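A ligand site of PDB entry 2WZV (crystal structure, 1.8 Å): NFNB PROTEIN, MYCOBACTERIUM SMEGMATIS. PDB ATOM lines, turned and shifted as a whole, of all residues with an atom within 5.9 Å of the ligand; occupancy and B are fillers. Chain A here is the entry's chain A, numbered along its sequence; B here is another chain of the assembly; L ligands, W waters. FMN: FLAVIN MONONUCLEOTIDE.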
ATOM      1  N   ARG A  26      35.321 -15.365 -27.507  1.00  0.00           N
ATOM      2  CA  ARG A  26      34.292 -16.391 -27.664  1.00  0.00           C
ATOM      3  C   ARG A  26      33.074 -16.002 -26.800  1.00  0.00           C
ATOM      4  O   ARG A  26      33.221 -15.732 -25.606  1.00  0.00           O
ATOM      5  CB  ARG A  26      34.823 -17.776 -27.223  1.00  0.00           C
ATOM      6  CG  ARG A  26      33.782 -18.929 -27.354  1.00  0.00           C
ATOM      7  CD  ARG A  26      33.686 -19.845 -26.135  1.00  0.00           C
ATOM      8  NE  ARG A  26      33.477 -19.100 -24.883  1.00  0.00           N
ATOM      9  CZ  ARG A  26      32.311 -18.631 -24.457  1.00  0.00           C
ATOM     10  NH1 ARG A  26      31.181 -18.876 -25.128  1.00  0.00           N
ATOM     11  NH2 ARG A  26      32.250 -17.909 -23.335  1.00  0.00           N
ATOM     12  N   ARG A  27      31.891 -15.954 -27.421  1.00  0.00           N
ATOM     13  CA  ARG A  27      30.631 -15.633 -26.734  1.00  0.00           C
ATOM     14  C   ARG A  27      29.554 -16.566 -27.272  1.00  0.00           C
ATOM     15  O   ARG A  27      29.713 -17.105 -28.358  1.00  0.00           O
ATOM     16  CB  ARG A  27      30.229 -14.149 -26.984  1.00  0.00           C
ATOM     17  CG  ARG A  27      31.141 -13.149 -26.272  1.00  0.00           C
ATOM     18  CD  ARG A  27      30.753 -11.722 -26.564  1.00  0.00           C
ATOM     19  NE  ARG A  27      31.832 -10.794 -26.190  1.00  0.00           N
ATOM     20  CZ  ARG A  27      32.747 -10.314 -27.029  1.00  0.00           C
ATOM     21  NH1 ARG A  27      32.736 -10.674 -28.305  1.00  0.00           N
ATOM     22  NH2 ARG A  27      33.672  -9.476 -26.593  1.00  0.00           N
ATOM     23  N   ALA A  28      28.443 -16.736 -26.524  1.00  0.00           N
ATOM     24  CA  ALA A  28      27.359 -17.584 -27.021  1.00  0.00           C
ATOM     25  C   ALA A  28      26.574 -16.711 -28.022  1.00  0.00           C
ATOM     26  O   ALA A  28      25.997 -15.687 -27.652  1.00  0.00           O
ATOM     27  CB  ALA A  28      26.463 -18.060 -25.880  1.00  0.00           C
ATOM     28  N   VAL A  29      26.680 -17.063 -29.305  1.00  0.00           N
ATOM     29  CA  VAL A  29      26.045 -16.320 -30.403  1.00  0.00           C
ATOM     30  C   VAL A  29      24.713 -16.966 -30.736  1.00  0.00           C
ATOM     31  O   VAL A  29      24.639 -18.179 -30.916  1.00  0.00           O
ATOM     32  CB  VAL A  29      27.038 -16.220 -31.595  1.00  0.00           C
ATOM     33  CG1 VAL A  29      26.340 -15.790 -32.890  1.00  0.00           C
ATOM     34  CG2 VAL A  29      28.182 -15.259 -31.252  1.00  0.00           C
ATOM     35  N   ARG A  30      23.659 -16.137 -30.805  1.00  0.00           N
ATOM     36  CA  ARG A  30      22.281 -16.624 -30.996  1.00  0.00           C
ATOM     37  C   ARG A  30      21.549 -16.063 -32.209  1.00  0.00           C
ATOM     38  O   ARG A  30      20.324 -16.050 -32.245  1.00  0.00           O
ATOM     39  CB  ARG A  30      21.472 -16.388 -29.694  1.00  0.00           C
ATOM     40  CG  ARG A  30      22.071 -17.128 -28.486  1.00  0.00           C
ATOM     41  CD  ARG A  30      21.306 -16.810 -27.208  1.00  0.00           C
ATOM     42  NE  ARG A  30      21.860 -17.568 -26.083  1.00  0.00           N
ATOM     43  CZ  ARG A  30      22.776 -17.105 -25.238  1.00  0.00           C
ATOM     44  NH1 ARG A  30      23.263 -15.868 -25.368  1.00  0.00           N
ATOM     45  NH2 ARG A  30      23.235 -17.873 -24.259  1.00  0.00           N
ATOM     46  N   PHE A 109      21.737 -14.227 -15.554  1.00  0.00           N
ATOM     47  CA  PHE A 109      21.967 -14.486 -16.975  1.00  0.00           C
ATOM     48  C   PHE A 109      20.632 -14.393 -17.770  1.00  0.00           C
ATOM     49  O   PHE A 109      20.572 -13.725 -18.804  1.00  0.00           O
ATOM     50  CB  PHE A 109      22.670 -15.842 -17.174  1.00  0.00           C
ATOM     51  CG  PHE A 109      22.338 -16.471 -18.511  1.00  0.00           C
ATOM     52  CD1 PHE A 109      22.846 -15.949 -19.691  1.00  0.00           C
ATOM     53  CD2 PHE A 109      21.504 -17.581 -18.579  1.00  0.00           C
ATOM     54  CE1 PHE A 109      22.495 -16.509 -20.937  1.00  0.00           C
ATOM     55  CE2 PHE A 109      21.161 -18.142 -19.810  1.00  0.00           C
ATOM     56  CZ  PHE A 109      21.669 -17.612 -20.983  1.00  0.00           C
ATOM     57  N   LEU A 113      19.685 -12.020 -20.933  1.00  0.00           N
ATOM     58  CA  LEU A 113      19.318 -12.595 -22.236  1.00  0.00           C
ATOM     59  C   LEU A 113      17.919 -12.147 -22.667  1.00  0.00           C
ATOM     60  O   LEU A 113      17.761 -11.644 -23.790  1.00  0.00           O
ATOM     61  CB  LEU A 113      19.417 -14.123 -22.177  1.00  0.00           C
ATOM     62  CG  LEU A 113      18.941 -14.880 -23.440  1.00  0.00           C
ATOM     63  CD1 LEU A 113      19.824 -14.544 -24.647  1.00  0.00           C
ATOM     64  CD2 LEU A 113      18.926 -16.374 -23.190  1.00  0.00           C
ATOM     65  N   TYR A 130      10.835 -18.092 -29.594  1.00  0.00           N
ATOM     66  CA  TYR A 130      12.280 -18.082 -29.333  1.00  0.00           C
ATOM     67  C   TYR A 130      12.857 -19.507 -29.190  1.00  0.00           C
ATOM     68  O   TYR A 130      13.924 -19.808 -29.738  1.00  0.00           O
ATOM     69  CB  TYR A 130      12.623 -17.173 -28.123  1.00  0.00           C
ATOM     70  CG  TYR A 130      14.070 -17.292 -27.713  1.00  0.00           C
ATOM     71  CD1 TYR A 130      15.083 -16.752 -28.496  1.00  0.00           C
ATOM     72  CD2 TYR A 130      14.435 -18.011 -26.579  1.00  0.00           C
ATOM     73  CE1 TYR A 130      16.432 -16.933 -28.155  1.00  0.00           C
ATOM     74  CE2 TYR A 130      15.765 -18.171 -26.214  1.00  0.00           C
ATOM     75  CZ  TYR A 130      16.758 -17.642 -27.013  1.00  0.00           C
ATOM     76  OH  TYR A 130      18.078 -17.799 -26.650  1.00  0.00           O
ATOM     77  N   SER A 134      15.652 -21.541 -31.378  1.00  0.00           N
ATOM     78  CA  SER A 134      16.797 -22.215 -30.761  1.00  0.00           C
ATOM     79  C   SER A 134      16.948 -23.658 -31.284  1.00  0.00           C
ATOM     80  O   SER A 134      18.066 -24.143 -31.471  1.00  0.00           O
ATOM     81  CB  SER A 134      16.686 -22.187 -29.239  1.00  0.00           C
ATOM     82  OG  SER A 134      16.351 -20.899 -28.758  1.00  0.00           O
ATOM     83  N   TYR A 138      19.435 -21.347 -34.157  1.00  0.00           N
ATOM     84  CA  TYR A 138      19.563 -19.896 -34.325  1.00  0.00           C
ATOM     85  C   TYR A 138      19.905 -19.465 -35.794  1.00  0.00           C
ATOM     86  O   TYR A 138      20.503 -18.408 -36.036  1.00  0.00           O
ATOM     87  CB  TYR A 138      20.561 -19.325 -33.309  1.00  0.00           C
ATOM     88  CG  TYR A 138      20.203 -19.565 -31.860  1.00  0.00           C
ATOM     89  CD1 TYR A 138      19.084 -18.980 -31.297  1.00  0.00           C
ATOM     90  CD2 TYR A 138      21.025 -20.342 -31.037  1.00  0.00           C
ATOM     91  CE1 TYR A 138      18.781 -19.131 -29.944  1.00  0.00           C
ATOM     92  CE2 TYR A 138      20.728 -20.509 -29.682  1.00  0.00           C
ATOM     93  CZ  TYR A 138      19.594 -19.915 -29.143  1.00  0.00           C
ATOM     94  OH  TYR A 138      19.276 -20.049 -27.808  1.00  0.00           O
ATOM     95  N   MET A 168      35.249 -24.874 -29.243  1.00  0.00           N
ATOM     96  CA  MET A 168      34.727 -23.503 -29.346  1.00  0.00           C
ATOM     97  C   MET A 168      35.848 -22.472 -29.528  1.00  0.00           C
ATOM     98  O   MET A 168      35.691 -21.489 -30.256  1.00  0.00           O
ATOM     99  CB  MET A 168      33.822 -23.172 -28.158  1.00  0.00           C
ATOM    100  CG  MET A 168      32.501 -23.935 -28.249  1.00  0.00           C
ATOM    101  SD  MET A 168      31.296 -23.363 -26.829  1.00  0.00           S
ATOM    102  CE  MET A 168      32.108 -24.312 -25.280  1.00  0.00           C
ATOM    103  N   CYS A 179      27.344 -21.407 -30.359  1.00  0.00           N
ATOM    104  CA  CYS A 179      26.491 -21.403 -29.182  1.00  0.00           C
ATOM    105  C   CYS A 179      26.383 -22.811 -28.651  1.00  0.00           C
ATOM    106  O   CYS A 179      25.779 -23.663 -29.326  1.00  0.00           O
ATOM    107  CB  CYS A 179      25.108 -20.815 -29.439  1.00  0.00           C
ATOM    108  SG  CYS A 179      24.168 -20.517 -27.915  1.00  0.00           S
ATOM    109  N   PRO A 180      26.924 -23.079 -27.448  1.00  0.00           N
ATOM    110  CA  PRO A 180      26.753 -24.409 -26.862  1.00  0.00           C
ATOM    111  C   PRO A 180      25.293 -24.489 -26.423  1.00  0.00           C
ATOM    112  O   PRO A 180      24.730 -23.456 -25.988  1.00  0.00           O
ATOM    113  CB  PRO A 180      27.721 -24.409 -25.684  1.00  0.00           C
ATOM    114  CG  PRO A 180      27.866 -22.980 -25.289  1.00  0.00           C
ATOM    115  CD  PRO A 180      27.680 -22.180 -26.538  1.00  0.00           C
ATOM    116  N   GLN A 181      24.635 -25.624 -26.668  1.00  0.00           N
ATOM    117  CA  GLN A 181      23.223 -25.693 -26.325  1.00  0.00           C
ATOM    118  C   GLN A 181      22.847 -26.972 -25.604  1.00  0.00           C
ATOM    119  O   GLN A 181      22.781 -28.030 -26.242  1.00  0.00           O
ATOM    120  CB  GLN A 181      22.356 -25.586 -27.608  1.00  0.00           C
ATOM    121  CG  GLN A 181      22.360 -24.222 -28.276  1.00  0.00           C
ATOM    122  CD  GLN A 181      21.535 -24.240 -29.542  1.00  0.00           C
ATOM    123  OE1 GLN A 181      22.052 -24.478 -30.621  1.00  0.00           O
ATOM    124  NE2 GLN A 181      20.240 -24.032 -29.427  1.00  0.00           N
ATOM    125  N   ALA A 182      22.523 -26.888 -24.306  1.00  0.00           N
ATOM    126  CA  ALA A 182      21.993 -28.065 -23.578  1.00  0.00           C
ATOM    127  C   ALA A 182      20.583 -28.381 -24.133  1.00  0.00           C
ATOM    128  O   ALA A 182      20.152 -29.530 -24.112  1.00  0.00           O
ATOM    129  CB  ALA A 182      21.886 -27.764 -22.082  1.00  0.00           C
ATOM    130  N   LEU A 183      19.875 -27.344 -24.625  1.00  0.00           N
ATOM    131  CA  LEU A 183      18.505 -27.550 -25.144  1.00  0.00           C
ATOM    132  C   LEU A 183      18.384 -28.716 -26.143  1.00  0.00           C
ATOM    133  O   LEU A 183      17.425 -29.482 -26.089  1.00  0.00           O
ATOM    134  CB  LEU A 183      17.990 -26.264 -25.781  1.00  0.00           C
ATOM    135  CG  LEU A 183      16.646 -26.397 -26.511  1.00  0.00           C
ATOM    136  CD1 LEU A 183      15.486 -26.675 -25.522  1.00  0.00           C
ATOM    137  CD2 LEU A 183      16.381 -25.176 -27.333  1.00  0.00           C
ATOM    138  N   LEU A 184      19.352 -28.824 -27.059  1.00  0.00           N
ATOM    139  CA  LEU A 184      19.355 -29.875 -28.084  1.00  0.00           C
ATOM    140  C   LEU A 184      19.426 -31.286 -27.509  1.00  0.00           C
ATOM    141  O   LEU A 184      18.889 -32.207 -28.112  1.00  0.00           O
ATOM    142  CB  LEU A 184      20.482 -29.611 -29.083  1.00  0.00           C
ATOM    143  CG  LEU A 184      20.483 -28.217 -29.754  1.00  0.00           C
ATOM    144  CD1 LEU A 184      21.666 -28.071 -30.684  1.00  0.00           C
ATOM    145  CD2 LEU A 184      19.166 -27.936 -30.523  1.00  0.00           C
ATOM    146  N   MET A 204      25.204 -32.369 -25.342  1.00  0.00           N
ATOM    147  CA  MET A 204      24.891 -31.019 -25.846  1.00  0.00           C
ATOM    148  C   MET A 204      25.110 -30.969 -27.349  1.00  0.00           C
ATOM    149  O   MET A 204      25.734 -31.873 -27.926  1.00  0.00           O
ATOM    150  CB  MET A 204      25.822 -29.961 -25.174  1.00  0.00           C
ATOM    151  CG  MET A 204      27.280 -29.990 -25.702  1.00  0.00           C
ATOM    152  SD  MET A 204      28.413 -28.561 -24.978  1.00  0.00           S
ATOM    153  CE  MET A 204      29.012 -29.498 -23.371  1.00  0.00           C
ATOM    154  N   VAL A 220      24.545  -8.745 -26.435  1.00  0.00           N
ATOM    155  CA  VAL A 220      24.517  -9.051 -25.011  1.00  0.00           C
ATOM    156  C   VAL A 220      25.939  -9.414 -24.529  1.00  0.00           C
ATOM    157  O   VAL A 220      26.705 -10.021 -25.269  1.00  0.00           O
ATOM    158  CB  VAL A 220      23.426 -10.097 -24.630  1.00  0.00           C
ATOM    159  CG1 VAL A 220      23.882 -11.528 -24.881  1.00  0.00           C
ATOM    160  CG2 VAL A 220      22.982  -9.937 -23.176  1.00  0.00           C
ATOM    161  N   ILE A 222      27.656 -11.049 -21.226  1.00  0.00           N
ATOM    162  CA  ILE A 222      27.403 -11.713 -19.958  1.00  0.00           C
ATOM    163  C   ILE A 222      28.629 -11.628 -19.065  1.00  0.00           C
ATOM    164  O   ILE A 222      29.704 -12.073 -19.461  1.00  0.00           O
ATOM    165  CB  ILE A 222      26.953 -13.178 -20.229  1.00  0.00           C
ATOM    166  CG1 ILE A 222      25.668 -13.241 -21.110  1.00  0.00           C
ATOM    167  CG2 ILE A 222      26.823 -13.964 -18.927  1.00  0.00           C
ATOM    168  CD1 ILE A 222      24.321 -12.566 -20.548  1.00  0.00           C
ATOM    169  N   ARG A 224      31.152 -12.152 -15.568  1.00  0.00           N
ATOM    170  CA  ARG A 224      31.615 -13.298 -14.780  1.00  0.00           C
ATOM    171  C   ARG A 224      31.727 -12.806 -13.348  1.00  0.00           C
ATOM    172  O   ARG A 224      31.825 -11.589 -13.116  1.00  0.00           O
ATOM    173  CB  ARG A 224      32.966 -13.825 -15.285  1.00  0.00           C
ATOM    174  CG  ARG A 224      32.880 -14.494 -16.667  1.00  0.00           C
ATOM    175  CD  ARG A 224      31.962 -15.737 -16.724  1.00  0.00           C
ATOM    176  NE  ARG A 224      32.141 -16.440 -17.991  1.00  0.00           N
ATOM    177  CZ  ARG A 224      31.488 -16.154 -19.109  1.00  0.00           C
ATOM    178  NH1 ARG A 224      30.557 -15.196 -19.112  1.00  0.00           N
ATOM    179  NH2 ARG A 224      31.750 -16.807 -20.228  1.00  0.00           N
ATOM    180  N   HIS B  51      36.583 -16.674 -17.562  1.00  0.00           N
ATOM    181  CA  HIS B  51      35.788 -16.389 -18.769  1.00  0.00           C
ATOM    182  C   HIS B  51      35.279 -17.624 -19.486  1.00  0.00           C
ATOM    183  O   HIS B  51      34.625 -17.522 -20.528  1.00  0.00           O
ATOM    184  CB  HIS B  51      36.498 -15.425 -19.718  1.00  0.00           C
ATOM    185  CG  HIS B  51      36.554 -14.049 -19.156  1.00  0.00           C
ATOM    186  ND1 HIS B  51      35.522 -13.154 -19.351  1.00  0.00           N
ATOM    187  CD2 HIS B  51      37.505 -13.469 -18.376  1.00  0.00           C
ATOM    188  CE1 HIS B  51      35.877 -12.047 -18.697  1.00  0.00           C
ATOM    189  NE2 HIS B  51      37.060 -12.199 -18.093  1.00  0.00           N
ATOM    190  N   ALA B  52      35.552 -18.801 -18.932  1.00  0.00           N
ATOM    191  CA  ALA B  52      34.981 -20.043 -19.449  1.00  0.00           C
ATOM    192  C   ALA B  52      33.420 -19.941 -19.456  1.00  0.00           C
ATOM    193  O   ALA B  52      32.846 -19.400 -18.507  1.00  0.00           O
ATOM    194  CB  ALA B  52      35.394 -21.206 -18.558  1.00  0.00           C
ATOM    195  N   PRO B  53      32.736 -20.464 -20.489  1.00  0.00           N
ATOM    196  CA  PRO B  53      31.275 -20.493 -20.464  1.00  0.00           C
ATOM    197  C   PRO B  53      30.788 -21.620 -19.521  1.00  0.00           C
ATOM    198  O   PRO B  53      31.579 -22.462 -19.082  1.00  0.00           O
ATOM    199  CB  PRO B  53      30.884 -20.775 -21.922  1.00  0.00           C
ATOM    200  CG  PRO B  53      32.019 -21.657 -22.417  1.00  0.00           C
ATOM    201  CD  PRO B  53      33.272 -21.082 -21.729  1.00  0.00           C
ATOM    202  N   SER B  54      29.486 -21.653 -19.233  1.00  0.00           N
ATOM    203  CA  SER B  54      28.905 -22.715 -18.401  1.00  0.00           C
ATOM    204  C   SER B  54      27.411 -22.664 -18.589  1.00  0.00           C
ATOM    205  O   SER B  54      26.907 -21.630 -19.056  1.00  0.00           O
ATOM    206  CB  SER B  54      29.254 -22.509 -16.912  1.00  0.00           C
ATOM    207  OG  SER B  54      28.906 -21.206 -16.464  1.00  0.00           O
ATOM    208  N   ASN B  55      26.714 -23.745 -18.199  1.00  0.00           N
ATOM    209  CA  ASN B  55      25.234 -23.783 -18.268  1.00  0.00           C
ATOM    210  C   ASN B  55      24.693 -22.578 -17.497  1.00  0.00           C
ATOM    211  O   ASN B  55      25.056 -22.420 -16.324  1.00  0.00           O
ATOM    212  CB  ASN B  55      24.692 -25.064 -17.618  1.00  0.00           C
ATOM    213  CG  ASN B  55      24.951 -26.279 -18.451  1.00  0.00           C
ATOM    214  OD1 ASN B  55      24.185 -26.613 -19.341  1.00  0.00           O
ATOM    215  ND2 ASN B  55      26.036 -27.013 -18.158  1.00  0.00           N
ATOM    216  N   SER B  56      23.955 -21.700 -18.170  1.00  0.00           N
ATOM    217  CA  SER B  56      23.293 -20.528 -17.547  1.00  0.00           C
ATOM    218  C   SER B  56      24.276 -19.582 -16.842  1.00  0.00           C
ATOM    219  O   SER B  56      23.871 -18.865 -15.919  1.00  0.00           O
ATOM    220  CB  SER B  56      22.266 -21.018 -16.527  1.00  0.00           C
ATOM    221  OG  SER B  56      21.201 -21.692 -17.168  1.00  0.00           O
ATOM    222  N   ASN B  57      25.556 -19.589 -17.251  1.00  0.00           N
ATOM    223  CA  ASN B  57      26.597 -18.764 -16.628  1.00  0.00           C
ATOM    224  C   ASN B  57      26.739 -19.074 -15.097  1.00  0.00           C
ATOM    225  O   ASN B  57      27.116 -18.197 -14.317  1.00  0.00           O
ATOM    226  CB  ASN B  57      26.335 -17.255 -16.877  1.00  0.00           C
ATOM    227  CG  ASN B  57      27.559 -16.407 -16.628  1.00  0.00           C
ATOM    228  OD1 ASN B  57      28.668 -16.787 -17.012  1.00  0.00           O
ATOM    229  ND2 ASN B  57      27.373 -15.259 -15.972  1.00  0.00           N
ATOM    230  N   ARG B 155      26.208 -32.735 -16.204  1.00  0.00           N
ATOM    231  CA  ARG B 155      26.177 -31.394 -16.809  1.00  0.00           C
ATOM    232  C   ARG B 155      27.110 -30.427 -16.078  1.00  0.00           C
ATOM    233  O   ARG B 155      27.870 -29.686 -16.726  1.00  0.00           O
ATOM    234  CB  ARG B 155      24.748 -30.855 -16.895  1.00  0.00           C
ATOM    235  CG  ARG B 155      23.871 -31.750 -17.749  1.00  0.00           C
ATOM    236  CD  ARG B 155      22.534 -31.109 -18.027  1.00  0.00           C
ATOM    237  NE  ARG B 155      21.684 -31.992 -18.836  1.00  0.00           N
ATOM    238  CZ  ARG B 155      21.727 -32.054 -20.156  1.00  0.00           C
ATOM    239  NH1 ARG B 155      22.573 -31.277 -20.840  1.00  0.00           N
ATOM    240  NH2 ARG B 155      20.962 -32.917 -20.813  1.00  0.00           N
ATOM    241  N   ASP B 159      30.915 -28.551 -17.293  1.00  0.00           N
ATOM    242  CA  ASP B 159      31.349 -27.161 -17.101  1.00  0.00           C
ATOM    243  C   ASP B 159      32.681 -27.085 -16.381  1.00  0.00           C
ATOM    244  O   ASP B 159      33.506 -26.219 -16.705  1.00  0.00           O
ATOM    245  CB  ASP B 159      30.274 -26.363 -16.361  1.00  0.00           C
ATOM    246  CG  ASP B 159      29.041 -26.103 -17.240  1.00  0.00           C
ATOM    247  OD1 ASP B 159      29.113 -26.348 -18.473  1.00  0.00           O
ATOM    248  OD2 ASP B 159      27.998 -25.734 -16.681  1.00  0.00           O
ATOM    249  N   ILE B 162      35.179 -27.621 -19.093  1.00  0.00           N
ATOM    250  CA  ILE B 162      35.320 -26.379 -19.896  1.00  0.00           C
ATOM    251  C   ILE B 162      36.287 -25.433 -19.144  1.00  0.00           C
ATOM    252  O   ILE B 162      37.270 -24.937 -19.719  1.00  0.00           O
ATOM    253  CB  ILE B 162      33.942 -25.737 -20.094  1.00  0.00           C
ATOM    254  CG1 ILE B 162      33.059 -26.587 -21.060  1.00  0.00           C
ATOM    255  CG2 ILE B 162      34.079 -24.268 -20.591  1.00  0.00           C
ATOM    256  CD1 ILE B 162      31.637 -26.011 -21.206  1.00  0.00           C
HETATM  257  N1  FMN L   1      22.698 -21.045 -24.254  1.00  0.00           N
HETATM  258  C2  FMN L   1      21.509 -21.157 -24.874  1.00  0.00           C
HETATM  259  O2  FMN L   1      20.993 -20.087 -25.490  1.00  0.00           O
HETATM  260  N3  FMN L   1      20.829 -22.329 -24.888  1.00  0.00           N
HETATM  261  C4  FMN L   1      21.346 -23.415 -24.300  1.00  0.00           C
HETATM  262  O4  FMN L   1      20.649 -24.561 -24.298  1.00  0.00           O
HETATM  263  C4A FMN L   1      22.564 -23.323 -23.631  1.00  0.00           C
HETATM  264  N5  FMN L   1      23.106 -24.439 -22.979  1.00  0.00           N
HETATM  265  C5A FMN L   1      24.482 -24.407 -22.629  1.00  0.00           C
HETATM  266  C6  FMN L   1      25.143 -25.580 -22.250  1.00  0.00           C
HETATM  267  C7  FMN L   1      26.504 -25.538 -21.924  1.00  0.00           C
HETATM  268  C7M FMN L   1      27.228 -26.842 -21.538  1.00  0.00           C
HETATM  269  C8  FMN L   1      27.202 -24.315 -21.955  1.00  0.00           C
HETATM  270  C8M FMN L   1      28.708 -24.236 -21.643  1.00  0.00           C
HETATM  271  C9  FMN L   1      26.527 -23.137 -22.307  1.00  0.00           C
HETATM  272  C9A FMN L   1      25.181 -23.185 -22.674  1.00  0.00           C
HETATM  273  N10 FMN L   1      24.504 -21.987 -23.050  1.00  0.00           N
HETATM  274  C10 FMN L   1      23.238 -22.091 -23.624  1.00  0.00           C
HETATM  275  C1' FMN L   1      25.292 -20.735 -23.296  1.00  0.00           C
HETATM  276  C2' FMN L   1      25.344 -19.813 -22.065  1.00  0.00           C
HETATM  277  O2' FMN L   1      24.353 -19.613 -21.347  1.00  0.00           O
HETATM  278  C3' FMN L   1      26.615 -18.962 -21.918  1.00  0.00           C
HETATM  279  O3' FMN L   1      27.820 -19.695 -22.241  1.00  0.00           O
HETATM  280  C4' FMN L   1      26.729 -18.235 -20.560  1.00  0.00           C
HETATM  281  O4' FMN L   1      25.568 -17.380 -20.430  1.00  0.00           O
HETATM  282  C5' FMN L   1      27.997 -17.366 -20.587  1.00  0.00           C
HETATM  283  O5' FMN L   1      27.887 -16.414 -21.685  1.00  0.00           O
HETATM  284  P   FMN L   1      28.978 -16.312 -22.829  1.00  0.00           P
HETATM  285  O1P FMN L   1      29.272 -17.777 -23.375  1.00  0.00           O
HETATM  286  O2P FMN L   1      28.267 -15.490 -23.994  1.00  0.00           O
HETATM  287  O3P FMN L   1      30.224 -15.663 -22.335  1.00  0.00           O
HETATM  288  O   HOH W   1      25.239 -16.043 -22.983  1.00  0.00           O
HETATM  289  O   HOH W   2      30.872 -13.243 -21.706  1.00  0.00           O
HETATM  290  O   HOH W   3      26.199 -14.424 -25.343  1.00  0.00           O
HETATM  291  O   HOH W   4      29.771 -28.543 -20.247  1.00  0.00           O
HETATM  292  O   HOH W   5      18.372 -19.664 -24.757  1.00  0.00           O
HETATM  293  O   HOH W   6      28.285 -12.701 -23.659  1.00  0.00           O
HETATM  294  O   HOH W   7      27.517 -29.473 -19.382  1.00  0.00           O
HETATM  295  O   HOH W   8      22.026 -25.027 -19.744  1.00  0.00           O
HETATM  296  O   HOH W   9      18.924 -22.572 -26.779  1.00  0.00           O
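The side-chain hydroxyl (OH) of Tyr 138 is in hydrogen-bond range of an oxygen (O2) of the ligand (2.9 Å). The backbone NH (N) of Leu 183 is in hydrogen-bond range of an oxygen (O4) of the ligand (2.9 Å). An oxygen (O2) of the ligand is in hydrogen-bond range of the guanidinium group (NE) of Arg 30 (2.7 Å). An oxygen (O2P) of the ligand lies within hydrogen-bond range of the backbone NH of Ala 28 (2.8 Å). N5 of the ligand sits at hydrogen-bond distance from N of Ala 182 (2.8 Å). The guanidinium group of Arg 224 is in salt-bridge range of an oxygen (O3P) of the ligand (2.8 Å). An oxygen (O1P) of the ligand is in salt-bridge range of the guanidinium group (NH1) of Arg 26, 2.8 Å away.
NH1 of Arg 224 sits at hydrogen-bond distance from OD1 of Asn 57 of chain B. NE2 of Gln 181 sits at hydrogen-bond distance from O of Ser 134, 3.0 Å away. The side-chain hydroxyl (OH) of Tyr 138 sits at hydrogen-bond distance from the side-chain hydroxyl (OG) of Ser 134. O of Tyr 130 is in hydrogen-bond range of OG of Ser 134 (2.8 Å). The guanidinium group (NH1) of Arg 224 is in hydrogen-bond range of the backbone carbonyl oxygen (O) of Ile 222. The backbone carbonyl oxygen (O) of His 51 of chain B is in hydrogen-bond range of the guanidinium group (NH2) of Arg 224, at 3.0 Å. OH of Tyr 138 sits at hydrogen-bond distance from OH of Tyr 130, at 2.8 Å. The backbone carbonyl oxygen of Ala 52 of chain B is in hydrogen-bond range of the guanidinium group of Arg 224, at 3.1 Å.
O of Pro 180 sits close to N10 of the ligand (3.3 Å). CA of Arg 27 touches O2P of the ligand (3.6 Å). CD1 of Phe 109 touches O4' of the ligand, at 3.2 Å. Tyr 130 touches the ligand. Cys 179 touches the ligand (SG to N1, 3.98 Å). Gln 181 touches the ligand (CA to O4, 3.5 Å). CE of Met 204 touches C7M of the ligand, at 3.7 Å. Ile 222 touches the ligand. Pro 53 of chain B touches the ligand (CB to O3', 3.3 Å). Ser 54 of chain B touches the ligand (CA to C8M, 3.6 Å). Asn 55 of chain B touches the ligand. Ser 56 of chain B touches the ligand. Asn 57 of chain B touches the ligand. Asp 159 of chain B touches the ligand (OD1 to C7M, 3.6 Å). Ile 162 of chain B touches the ligand. Hydrophobic or aromatic side chains within 4 Å of the ligand: Ala 28, Phe 109, Tyr 138, Pro 180, Ala 182, Leu 183, Met 204, Ile 222, Pro 53 of chain B and Ile 162 of chain B. Of the 31 residues printed, 22 come within 4 Å of the ligand.
Water W2 lies within hydrogen-bond range of an oxygen (O3P) of the ligand (2.6 Å), the backbone carbonyl oxygen (O) of Ile 222 (2.8 Å) and the guanidinium group (NH1) of Arg 224 (3.3 Å). Water W3 lies within hydrogen-bond range of the backbone carbonyl oxygen of Ala 28 (2.6 Å), an oxygen (O2P) of the ligand (2.7 Å) and the guanidinium group of Arg 30 (3.3 Å). Water W9 lies within hydrogen-bond range of a nitrogen (N3) of the ligand (2.7 Å), the side-chain hydroxyl (OH) of Tyr 138 (2.7 Å) and the side-chain amide nitrogen (NE2) of Gln 181 (3.3 Å). Water W5 lies within hydrogen-bond range of the side-chain hydroxyl of Tyr 130 (2.7 Å), an oxygen (O2) of the ligand (2.8 Å) and the side-chain hydroxyl of Tyr 138 (3.2 Å). Water W6 lies within hydrogen-bond range of O2P of the ligand and N of Ile 222. Water W7 bridges O of Arg 155 of chain B (2.7 Å) and ND2 of Asn 55 of chain B (3.1 Å).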
